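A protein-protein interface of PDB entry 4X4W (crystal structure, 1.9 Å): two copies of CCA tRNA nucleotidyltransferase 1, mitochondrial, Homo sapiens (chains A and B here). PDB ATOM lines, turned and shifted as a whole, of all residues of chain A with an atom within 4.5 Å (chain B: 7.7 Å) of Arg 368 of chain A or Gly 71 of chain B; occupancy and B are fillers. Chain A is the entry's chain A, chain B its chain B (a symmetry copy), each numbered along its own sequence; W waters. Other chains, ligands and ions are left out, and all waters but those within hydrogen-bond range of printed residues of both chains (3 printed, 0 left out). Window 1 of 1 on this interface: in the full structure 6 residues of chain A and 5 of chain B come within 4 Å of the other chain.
Of the 10 printed residues of chain A, 4 touch a printed residue of chain B.
Of the 18 printed residues of chain B, 3 touch a printed residue of chain A.
Among the printed residues, 6 pairs touch across the chains.
Among the printed residues, no Asp or Glu carboxylate lies within 4 Å of a Lys or Arg side-chain nitrogen of the other chain.
Water W3 lies within hydrogen-bond range of NH1 of Arg 368 of chain A (2.4 Å) and O of Ala 70 of chain B (2.6 Å).
Water W2 lies within hydrogen-bond range of the backbone carbonyl oxygen (O) of Arg 88 of chain B, the backbone NH (N) of Arg 73 of chain B and a ring nitrogen (ND1) of His 365 of chain A.
Water W1 lies within hydrogen-bond range of N of His 365 of chain A (2.9 Å), O of Gly 71 of chain B (3.3 Å) and N of Gly 364 of chain A (3.5 Å).
Printed residues of chain B within 4 Å of Gly 364 of chain A: Gly 71.
Of the printed residues of chain B, His 365 of chain A touches Gly 71 and Arg 73.
Of chain B, only Ala 70 (3.5 Å) and Gly 71 (3.3 Å) come within 4 Å of Arg 368 of chain A.
Of the printed residues of chain B, Ile 378 of chain A touches Ala 70 (3.4 Å).
Gly 18 of chain B touches none of the printed residues of chain A.
Of the printed residues of chain A, Ala 70 of chain B touches Arg 368 and Ile 378.
Of chain A, only Gly 364, His 365 and Arg 368 come within 4 Å of Gly 71 of chain B.
Printed residues of chain A within 4 Å of Arg 73 of chain B: His 365 (2.9 Å).
His 90 of chain B touches none of the printed residues of chain A.
The nearest residue of chain B that does not touch Arg 368 of chain A is His 90 of chain B (4.1 Å).
The nearest printed residue of chain A that does not touch Gly 71 of chain B is Ile 378 of chain A (4.6 Å).
The nearest printed residue of chain B that does not touch Gly 364 of chain A is Ala 70 of chain B (5.4 Å).
No position is printed for both chains.
The backbone NH (N) of Arg 88 of chain B lies within hydrogen-bond range of the backbone carbonyl oxygen (O) of Arg 73 of chain B, at 3.0 Å.
Among the printed residues, pairs that only touch across the chains: Gly 364 of chain A with Gly 71 of chain B (3.4 Å), Arg 368 of chain A with Ala 70 of chain B (3.5 Å), Arg 368 of chain A with Gly 71 of chain B (3.3 Å) and Ile 378 of chain A with Ala 70 of chain B (3.4 Å).
NE2 of His 365 of chain A sits close to NH1 of Arg 73 of chain B (3.3 Å).
The backbone carbonyl oxygen (O) of Gly 71 of chain B is in hydrogen-bond range of the backbone NH (N) of His 365 of chain A.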
ATOM      1  N   GLY A 364     -15.441  -9.709  -5.238  1.00  0.00           N
ATOM      2  CA  GLY A 364     -16.704  -8.984  -5.298  1.00  0.00           C
ATOM      3  C   GLY A 364     -17.847  -9.695  -4.570  1.00  0.00           C
ATOM      4  O   GLY A 364     -18.644  -9.069  -3.897  1.00  0.00           O
ATOM      5  N   HIS A 365     -17.894 -11.019  -4.683  1.00  0.00           N
ATOM      6  CA  HIS A 365     -18.893 -11.838  -4.011  1.00  0.00           C
ATOM      7  C   HIS A 365     -18.829 -11.721  -2.491  1.00  0.00           C
ATOM      8  O   HIS A 365     -19.857 -11.743  -1.821  1.00  0.00           O
ATOM      9  CB  HIS A 365     -18.690 -13.295  -4.377  1.00  0.00           C
ATOM     10  CG  HIS A 365     -19.345 -14.248  -3.426  1.00  0.00           C
ATOM     11  ND1 HIS A 365     -20.724 -14.349  -3.303  1.00  0.00           N
ATOM     12  CD2 HIS A 365     -18.820 -15.154  -2.567  1.00  0.00           C
ATOM     13  CE1 HIS A 365     -21.013 -15.266  -2.396  1.00  0.00           C
ATOM     14  NE2 HIS A 365     -19.879 -15.774  -1.941  1.00  0.00           N
ATOM     15  N   ASP A 366     -17.625 -11.617  -1.961  1.00  0.00           N
ATOM     16  CA  ASP A 366     -17.414 -11.491  -0.515  1.00  0.00           C
ATOM     17  C   ASP A 366     -18.096 -10.213  -0.054  1.00  0.00           C
ATOM     18  O   ASP A 366     -18.756 -10.186   0.999  1.00  0.00           O
ATOM     19  CB  ASP A 366     -15.916 -11.432  -0.188  1.00  0.00           C
ATOM     20  CG  ASP A 366     -15.229 -12.789  -0.285  1.00  0.00           C
ATOM     21  OD1 ASP A 366     -15.899 -13.796   0.003  1.00  0.00           O
ATOM     22  OD2 ASP A 366     -14.015 -12.840  -0.643  1.00  0.00           O
ATOM     23  N   ILE A 367     -17.978  -9.158  -0.866  1.00  0.00           N
ATOM     24  CA  ILE A 367     -18.610  -7.896  -0.532  1.00  0.00           C
ATOM     25  C   ILE A 367     -20.114  -7.980  -0.730  1.00  0.00           C
ATOM     26  O   ILE A 367     -20.869  -7.400   0.036  1.00  0.00           O
ATOM     27  CB  ILE A 367     -18.017  -6.717  -1.357  1.00  0.00           C
ATOM     28  CG1 ILE A 367     -16.506  -6.641  -1.190  1.00  0.00           C
ATOM     29  CG2 ILE A 367     -18.664  -5.359  -0.967  1.00  0.00           C
ATOM     30  CD1 ILE A 367     -16.067  -6.376   0.257  1.00  0.00           C
ATOM     31  N   ARG A 368     -20.587  -8.673  -1.763  1.00  0.00           N
ATOM     32  CA  ARG A 368     -22.021  -8.785  -1.907  1.00  0.00           C
ATOM     33  C   ARG A 368     -22.652  -9.470  -0.687  1.00  0.00           C
ATOM     34  O   ARG A 368     -23.772  -9.143  -0.284  1.00  0.00           O
ATOM     35  CB  ARG A 368     -22.393  -9.596  -3.128  1.00  0.00           C
ATOM     36  CG  ARG A 368     -22.075  -8.937  -4.402  1.00  0.00           C
ATOM     37  CD  ARG A 368     -22.582  -9.789  -5.564  1.00  0.00           C
ATOM     38  NE  ARG A 368     -23.789 -10.518  -5.218  1.00  0.00           N
ATOM     39  CZ  ARG A 368     -25.029 -10.105  -5.492  1.00  0.00           C
ATOM     40  NH1 ARG A 368     -25.239  -8.948  -6.129  1.00  0.00           N
ATOM     41  NH2 ARG A 368     -26.065 -10.857  -5.123  1.00  0.00           N
ATOM     42  N   LYS A 369     -21.920 -10.428  -0.132  1.00  0.00           N
ATOM     43  CA  LYS A 369     -22.373 -11.186   1.023  1.00  0.00           C
ATOM     44  C   LYS A 369     -22.515 -10.330   2.293  1.00  0.00           C
ATOM     45  O   LYS A 369     -23.281 -10.680   3.169  1.00  0.00           O
ATOM     46  CB  LYS A 369     -21.437 -12.375   1.278  1.00  0.00           C
ATOM     47  CG  LYS A 369     -22.158 -13.610   1.743  1.00  0.00           C
ATOM     48  CD  LYS A 369     -21.330 -14.862   1.537  1.00  0.00           C
ATOM     49  CE  LYS A 369     -22.129 -16.135   1.877  1.00  0.00           C
ATOM     50  NZ  LYS A 369     -21.346 -17.397   1.636  1.00  0.00           N
ATOM     51  N   VAL A 370     -21.800  -9.216   2.399  1.00  0.00           N
ATOM     52  CA  VAL A 370     -21.951  -8.356   3.571  1.00  0.00           C
ATOM     53  C   VAL A 370     -23.105  -7.375   3.366  1.00  0.00           C
ATOM     54  O   VAL A 370     -23.363  -6.531   4.218  1.00  0.00           O
ATOM     55  CB  VAL A 370     -20.622  -7.601   3.957  1.00  0.00           C
ATOM     56  CG1 VAL A 370     -19.407  -8.502   3.786  1.00  0.00           C
ATOM     57  CG2 VAL A 370     -20.433  -6.334   3.156  1.00  0.00           C
ATOM     58  N   GLY A 371     -23.792  -7.483   2.230  1.00  0.00           N
ATOM     59  CA  GLY A 371     -24.993  -6.697   1.970  1.00  0.00           C
ATOM     60  C   GLY A 371     -24.929  -5.610   0.904  1.00  0.00           C
ATOM     61  O   GLY A 371     -25.897  -4.879   0.708  1.00  0.00           O
ATOM     62  N   ILE A 372     -23.809  -5.505   0.196  1.00  0.00           N
ATOM     63  CA  ILE A 372     -23.633  -4.467  -0.818  1.00  0.00           C
ATOM     64  C   ILE A 372     -24.049  -4.997  -2.166  1.00  0.00           C
ATOM     65  O   ILE A 372     -23.698  -6.107  -2.528  1.00  0.00           O
ATOM     66  CB  ILE A 372     -22.153  -4.046  -0.944  1.00  0.00           C
ATOM     67  CG1 ILE A 372     -21.528  -3.839   0.440  1.00  0.00           C
ATOM     68  CG2 ILE A 372     -22.038  -2.805  -1.812  1.00  0.00           C
ATOM     69  CD1 ILE A 372     -22.239  -2.766   1.287  1.00  0.00           C
ATOM     70  N   ILE A 378     -19.185  -1.775  -4.504  1.00  0.00           N
ATOM     71  CA  ILE A 378     -18.304  -2.948  -4.390  1.00  0.00           C
ATOM     72  C   ILE A 378     -16.853  -2.622  -4.808  1.00  0.00           C
ATOM     73  O   ILE A 378     -15.896  -3.005  -4.119  1.00  0.00           O
ATOM     74  CB  ILE A 378     -18.842  -4.125  -5.229  1.00  0.00           C
ATOM     75  CG1 ILE A 378     -20.063  -4.722  -4.565  1.00  0.00           C
ATOM     76  CG2 ILE A 378     -17.803  -5.218  -5.355  1.00  0.00           C
ATOM     77  CD1 ILE A 378     -20.946  -5.540  -5.501  1.00  0.00           C
ATOM     78  N   GLU B  17     -34.328 -16.451  -3.702  1.00  0.00           N
ATOM     79  CA  GLU B  17     -33.625 -15.183  -3.593  1.00  0.00           C
ATOM     80  C   GLU B  17     -32.664 -14.995  -4.775  1.00  0.00           C
ATOM     81  O   GLU B  17     -32.497 -13.867  -5.308  1.00  0.00           O
ATOM     82  CB  GLU B  17     -32.795 -15.129  -2.290  1.00  0.00           C
ATOM     83  CG  GLU B  17     -33.598 -14.911  -1.044  1.00  0.00           C
ATOM     84  CD  GLU B  17     -32.683 -14.625   0.141  1.00  0.00           C
ATOM     85  OE1 GLU B  17     -31.501 -14.277  -0.120  1.00  0.00           O
ATOM     86  OE2 GLU B  17     -33.134 -14.757   1.313  1.00  0.00           O
ATOM     87  N   GLY B  18     -32.039 -16.100  -5.160  1.00  0.00           N
ATOM     88  CA  GLY B  18     -31.138 -16.122  -6.295  1.00  0.00           C
ATOM     89  C   GLY B  18     -31.789 -15.733  -7.597  1.00  0.00           C
ATOM     90  O   GLY B  18     -31.272 -14.930  -8.334  1.00  0.00           O
ATOM     91  N   SER B  21     -32.740 -12.098  -7.668  1.00  0.00           N
ATOM     92  CA  SER B  21     -31.599 -11.258  -7.891  1.00  0.00           C
ATOM     93  C   SER B  21     -31.229 -11.291  -9.378  1.00  0.00           C
ATOM     94  O   SER B  21     -30.975 -10.252  -9.974  1.00  0.00           O
ATOM     95  CB  SER B  21     -30.413 -11.723  -7.063  1.00  0.00           C
ATOM     96  OG  SER B  21     -30.611 -11.373  -5.746  1.00  0.00           O
ATOM     97  N   LEU B  22     -31.210 -12.480  -9.967  1.00  0.00           N
ATOM     98  CA  LEU B  22     -30.808 -12.622 -11.370  1.00  0.00           C
ATOM     99  C   LEU B  22     -31.754 -11.867 -12.327  1.00  0.00           C
ATOM    100  O   LEU B  22     -31.303 -11.180 -13.264  1.00  0.00           O
ATOM    101  CB  LEU B  22     -30.827 -14.082 -11.765  1.00  0.00           C
ATOM    102  CG  LEU B  22     -30.358 -14.411 -13.185  1.00  0.00           C
ATOM    103  CD1 LEU B  22     -28.885 -14.126 -13.281  1.00  0.00           C
ATOM    104  CD2 LEU B  22     -30.689 -15.851 -13.599  1.00  0.00           C
ATOM    105  N   LEU B  25     -31.339  -8.123 -12.196  1.00  0.00           N
ATOM    106  CA  LEU B  25     -30.127  -7.680 -12.837  1.00  0.00           C
ATOM    107  C   LEU B  25     -30.378  -7.520 -14.359  1.00  0.00           C
ATOM    108  O   LEU B  25     -29.974  -6.538 -14.965  1.00  0.00           O
ATOM    109  CB  LEU B  25     -28.981  -8.683 -12.579  1.00  0.00           C
ATOM    110  CG  LEU B  25     -27.640  -8.424 -13.254  1.00  0.00           C
ATOM    111  CD1 LEU B  25     -27.047  -7.112 -12.798  1.00  0.00           C
ATOM    112  CD2 LEU B  25     -26.702  -9.587 -12.926  1.00  0.00           C
ATOM    113  N   GLU B  65     -19.369  -9.277 -18.741  1.00  0.00           N
ATOM    114  CA  GLU B  65     -19.182  -7.892 -18.266  1.00  0.00           C
ATOM    115  C   GLU B  65     -20.206  -7.482 -17.181  1.00  0.00           C
ATOM    116  O   GLU B  65     -19.871  -6.813 -16.235  1.00  0.00           O
ATOM    117  CB  GLU B  65     -19.220  -6.885 -19.442  1.00  0.00           C
ATOM    118  CG  GLU B  65     -17.973  -6.966 -20.342  1.00  0.00           C
ATOM    119  CD  GLU B  65     -18.151  -6.279 -21.699  1.00  0.00           C
ATOM    120  OE1 GLU B  65     -19.297  -5.889 -22.043  1.00  0.00           O
ATOM    121  OE2 GLU B  65     -17.146  -6.170 -22.434  1.00  0.00           O
ATOM    122  N   MET B  66     -21.449  -7.910 -17.333  1.00  0.00           N
ATOM    123  CA  MET B  66     -22.511  -7.652 -16.357  1.00  0.00           C
ATOM    124  C   MET B  66     -22.202  -8.302 -15.013  1.00  0.00           C
ATOM    125  O   MET B  66     -22.299  -7.661 -13.974  1.00  0.00           O
ATOM    126  CB  MET B  66     -23.812  -8.227 -16.932  1.00  0.00           C
ATOM    127  CG  MET B  66     -25.075  -7.895 -16.222  1.00  0.00           C
ATOM    128  SD  MET B  66     -26.578  -8.587 -17.052  1.00  0.00           S
ATOM    129  CE  MET B  66     -25.931  -8.723 -18.735  1.00  0.00           C
ATOM    130  N   PHE B  67     -21.861  -9.577 -15.019  1.00  0.00           N
ATOM    131  CA  PHE B  67     -21.522 -10.280 -13.768  1.00  0.00           C
ATOM    132  C   PHE B  67     -20.275  -9.735 -13.136  1.00  0.00           C
ATOM    133  O   PHE B  67     -20.257  -9.469 -11.940  1.00  0.00           O
ATOM    134  CB  PHE B  67     -21.427 -11.785 -14.001  1.00  0.00           C
ATOM    135  CG  PHE B  67     -22.765 -12.413 -14.414  1.00  0.00           C
ATOM    136  CD1 PHE B  67     -23.891 -12.214 -13.636  1.00  0.00           C
ATOM    137  CD2 PHE B  67     -22.868 -13.228 -15.552  1.00  0.00           C
ATOM    138  CE1 PHE B  67     -25.133 -12.795 -13.996  1.00  0.00           C
ATOM    139  CE2 PHE B  67     -24.102 -13.767 -15.941  1.00  0.00           C
ATOM    140  CZ  PHE B  67     -25.223 -13.576 -15.164  1.00  0.00           C
ATOM    141  N   GLN B  68     -19.231  -9.498 -13.921  1.00  0.00           N
ATOM    142  CA  GLN B  68     -17.989  -8.955 -13.341  1.00  0.00           C
ATOM    143  C   GLN B  68     -18.215  -7.567 -12.739  1.00  0.00           C
ATOM    144  O   GLN B  68     -17.730  -7.249 -11.652  1.00  0.00           O
ATOM    145  CB  GLN B  68     -16.892  -8.875 -14.413  1.00  0.00           C
ATOM    146  CG  GLN B  68     -16.313 -10.210 -14.822  1.00  0.00           C
ATOM    147  CD  GLN B  68     -15.492 -10.116 -16.097  1.00  0.00           C
ATOM    148  OE1 GLN B  68     -15.431  -9.055 -16.733  1.00  0.00           O
ATOM    149  NE2 GLN B  68     -14.850 -11.222 -16.479  1.00  0.00           N
ATOM    150  N   SER B  69     -18.947  -6.736 -13.459  1.00  0.00           N
ATOM    151  CA  SER B  69     -19.264  -5.367 -13.053  1.00  0.00           C
ATOM    152  C   SER B  69     -20.096  -5.331 -11.771  1.00  0.00           C
ATOM    153  O   SER B  69     -20.018  -4.367 -11.009  1.00  0.00           O
ATOM    154  CB  SER B  69     -20.010  -4.676 -14.208  1.00  0.00           C
ATOM    155  OG  SER B  69     -20.358  -3.344 -13.906  1.00  0.00           O
ATOM    156  N   ALA B  70     -20.858  -6.388 -11.510  1.00  0.00           N
ATOM    157  CA  ALA B  70     -21.713  -6.480 -10.317  1.00  0.00           C
ATOM    158  C   ALA B  70     -21.105  -7.331  -9.176  1.00  0.00           C
ATOM    159  O   ALA B  70     -21.724  -7.506  -8.107  1.00  0.00           O
ATOM    160  CB  ALA B  70     -23.014  -7.070 -10.729  1.00  0.00           C
ATOM    161  N   GLY B  71     -19.886  -7.853  -9.381  1.00  0.00           N
ATOM    162  CA  GLY B  71     -19.259  -8.682  -8.380  1.00  0.00           C
ATOM    163  C   GLY B  71     -19.930 -10.033  -8.206  1.00  0.00           C
ATOM    164  O   GLY B  71     -19.846 -10.623  -7.125  1.00  0.00           O
ATOM    165  N   ILE B  72     -20.569 -10.537  -9.264  1.00  0.00           N
ATOM    166  CA  ILE B  72     -21.245 -11.829  -9.247  1.00  0.00           C
ATOM    167  C   ILE B  72     -20.356 -12.952  -9.797  1.00  0.00           C
ATOM    168  O   ILE B  72     -19.862 -12.848 -10.896  1.00  0.00           O
ATOM    169  CB  ILE B  72     -22.563 -11.761 -10.107  1.00  0.00           C
ATOM    170  CG1 ILE B  72     -23.586 -10.885  -9.410  1.00  0.00           C
ATOM    171  CG2 ILE B  72     -23.210 -13.132 -10.308  1.00  0.00           C
ATOM    172  CD1 ILE B  72     -24.823 -10.585 -10.320  1.00  0.00           C
ATOM    173  N   ARG B  73     -20.179 -14.028  -9.029  1.00  0.00           N
ATOM    174  CA  ARG B  73     -19.297 -15.143  -9.422  1.00  0.00           C
ATOM    175  C   ARG B  73     -19.799 -15.855 -10.660  1.00  0.00           C
ATOM    176  O   ARG B  73     -20.987 -16.112 -10.798  1.00  0.00           O
ATOM    177  CB  ARG B  73     -19.201 -16.191  -8.308  1.00  0.00           C
ATOM    178  CG  ARG B  73     -18.368 -15.786  -7.176  1.00  0.00           C
ATOM    179  CD  ARG B  73     -18.543 -16.738  -5.983  1.00  0.00           C
ATOM    180  NE  ARG B  73     -19.928 -16.743  -5.522  1.00  0.00           N
ATOM    181  CZ  ARG B  73     -20.408 -17.532  -4.571  1.00  0.00           C
ATOM    182  NH1 ARG B  73     -19.616 -18.405  -3.942  1.00  0.00           N
ATOM    183  NH2 ARG B  73     -21.689 -17.433  -4.254  1.00  0.00           N
ATOM    184  N   MET B  74     -18.894 -16.186 -11.572  1.00  0.00           N
ATOM    185  CA  MET B  74     -19.263 -17.083 -12.657  1.00  0.00           C
ATOM    186  C   MET B  74     -18.515 -18.386 -12.440  1.00  0.00           C
ATOM    187  O   MET B  74     -17.434 -18.403 -11.863  1.00  0.00           O
ATOM    188  CB  MET B  74     -18.963 -16.477 -14.021  1.00  0.00           C
ATOM    189  CG  MET B  74     -19.766 -15.210 -14.287  1.00  0.00           C
ATOM    190  SD  MET B  74     -19.155 -14.424 -15.774  1.00  0.00           S
ATOM    191  CE  MET B  74     -17.787 -13.516 -15.071  1.00  0.00           C
ATOM    192  N   ARG B  88     -23.399 -17.760 -10.181  1.00  0.00           N
ATOM    193  CA  ARG B  88     -23.848 -18.197  -8.872  1.00  0.00           C
ATOM    194  C   ARG B  88     -24.322 -16.979  -8.094  1.00  0.00           C
ATOM    195  O   ARG B  88     -23.600 -15.977  -7.958  1.00  0.00           O
ATOM    196  CB  ARG B  88     -22.706 -18.901  -8.143  1.00  0.00           C
ATOM    197  CG  ARG B  88     -23.020 -19.365  -6.734  1.00  0.00           C
ATOM    198  CD  ARG B  88     -22.000 -20.362  -6.315  1.00  0.00           C
ATOM    199  NE  ARG B  88     -22.334 -21.060  -5.067  1.00  0.00           N
ATOM    200  CZ  ARG B  88     -23.109 -22.137  -4.969  1.00  0.00           C
ATOM    201  NH1 ARG B  88     -23.668 -22.686  -6.042  1.00  0.00           N
ATOM    202  NH2 ARG B  88     -23.312 -22.682  -3.768  1.00  0.00           N
ATOM    203  N   LEU B  89     -25.559 -17.049  -7.617  1.00  0.00           N
ATOM    204  CA  LEU B  89     -26.131 -16.026  -6.762  1.00  0.00           C
ATOM    205  C   LEU B  89     -26.931 -16.713  -5.678  1.00  0.00           C
ATOM    206  O   LEU B  89     -27.676 -17.639  -5.966  1.00  0.00           O
ATOM    207  CB  LEU B  89     -27.088 -15.095  -7.540  1.00  0.00           C
ATOM    208  CG  LEU B  89     -26.648 -14.256  -8.741  1.00  0.00           C
ATOM    209  CD1 LEU B  89     -26.614 -15.099 -10.006  1.00  0.00           C
ATOM    210  CD2 LEU B  89     -27.591 -13.085  -8.975  1.00  0.00           C
ATOM    211  N   HIS B  90     -26.782 -16.231  -4.438  1.00  0.00           N
ATOM    212  CA  HIS B  90     -27.479 -16.768  -3.263  1.00  0.00           C
ATOM    213  C   HIS B  90     -27.461 -18.291  -3.194  1.00  0.00           C
ATOM    214  O   HIS B  90     -28.492 -18.944  -3.113  1.00  0.00           O
ATOM    215  CB  HIS B  90     -28.900 -16.231  -3.207  1.00  0.00           C
ATOM    216  CG  HIS B  90     -28.959 -14.744  -3.047  1.00  0.00           C
ATOM    217  ND1 HIS B  90     -28.407 -14.091  -1.960  1.00  0.00           N
ATOM    218  CD2 HIS B  90     -29.480 -13.784  -3.843  1.00  0.00           C
ATOM    219  CE1 HIS B  90     -28.593 -12.787  -2.092  1.00  0.00           C
ATOM    220  NE2 HIS B  90     -29.236 -12.576  -3.231  1.00  0.00           N
HETATM  221  O   HOH W   1     -16.958 -12.229  -7.092  1.00  0.00           O
HETATM  222  O   HOH W   2     -21.763 -14.485  -6.557  1.00  0.00           O
HETATM  223  O   HOH W   3     -24.043  -7.065  -7.140  1.00  0.00           O
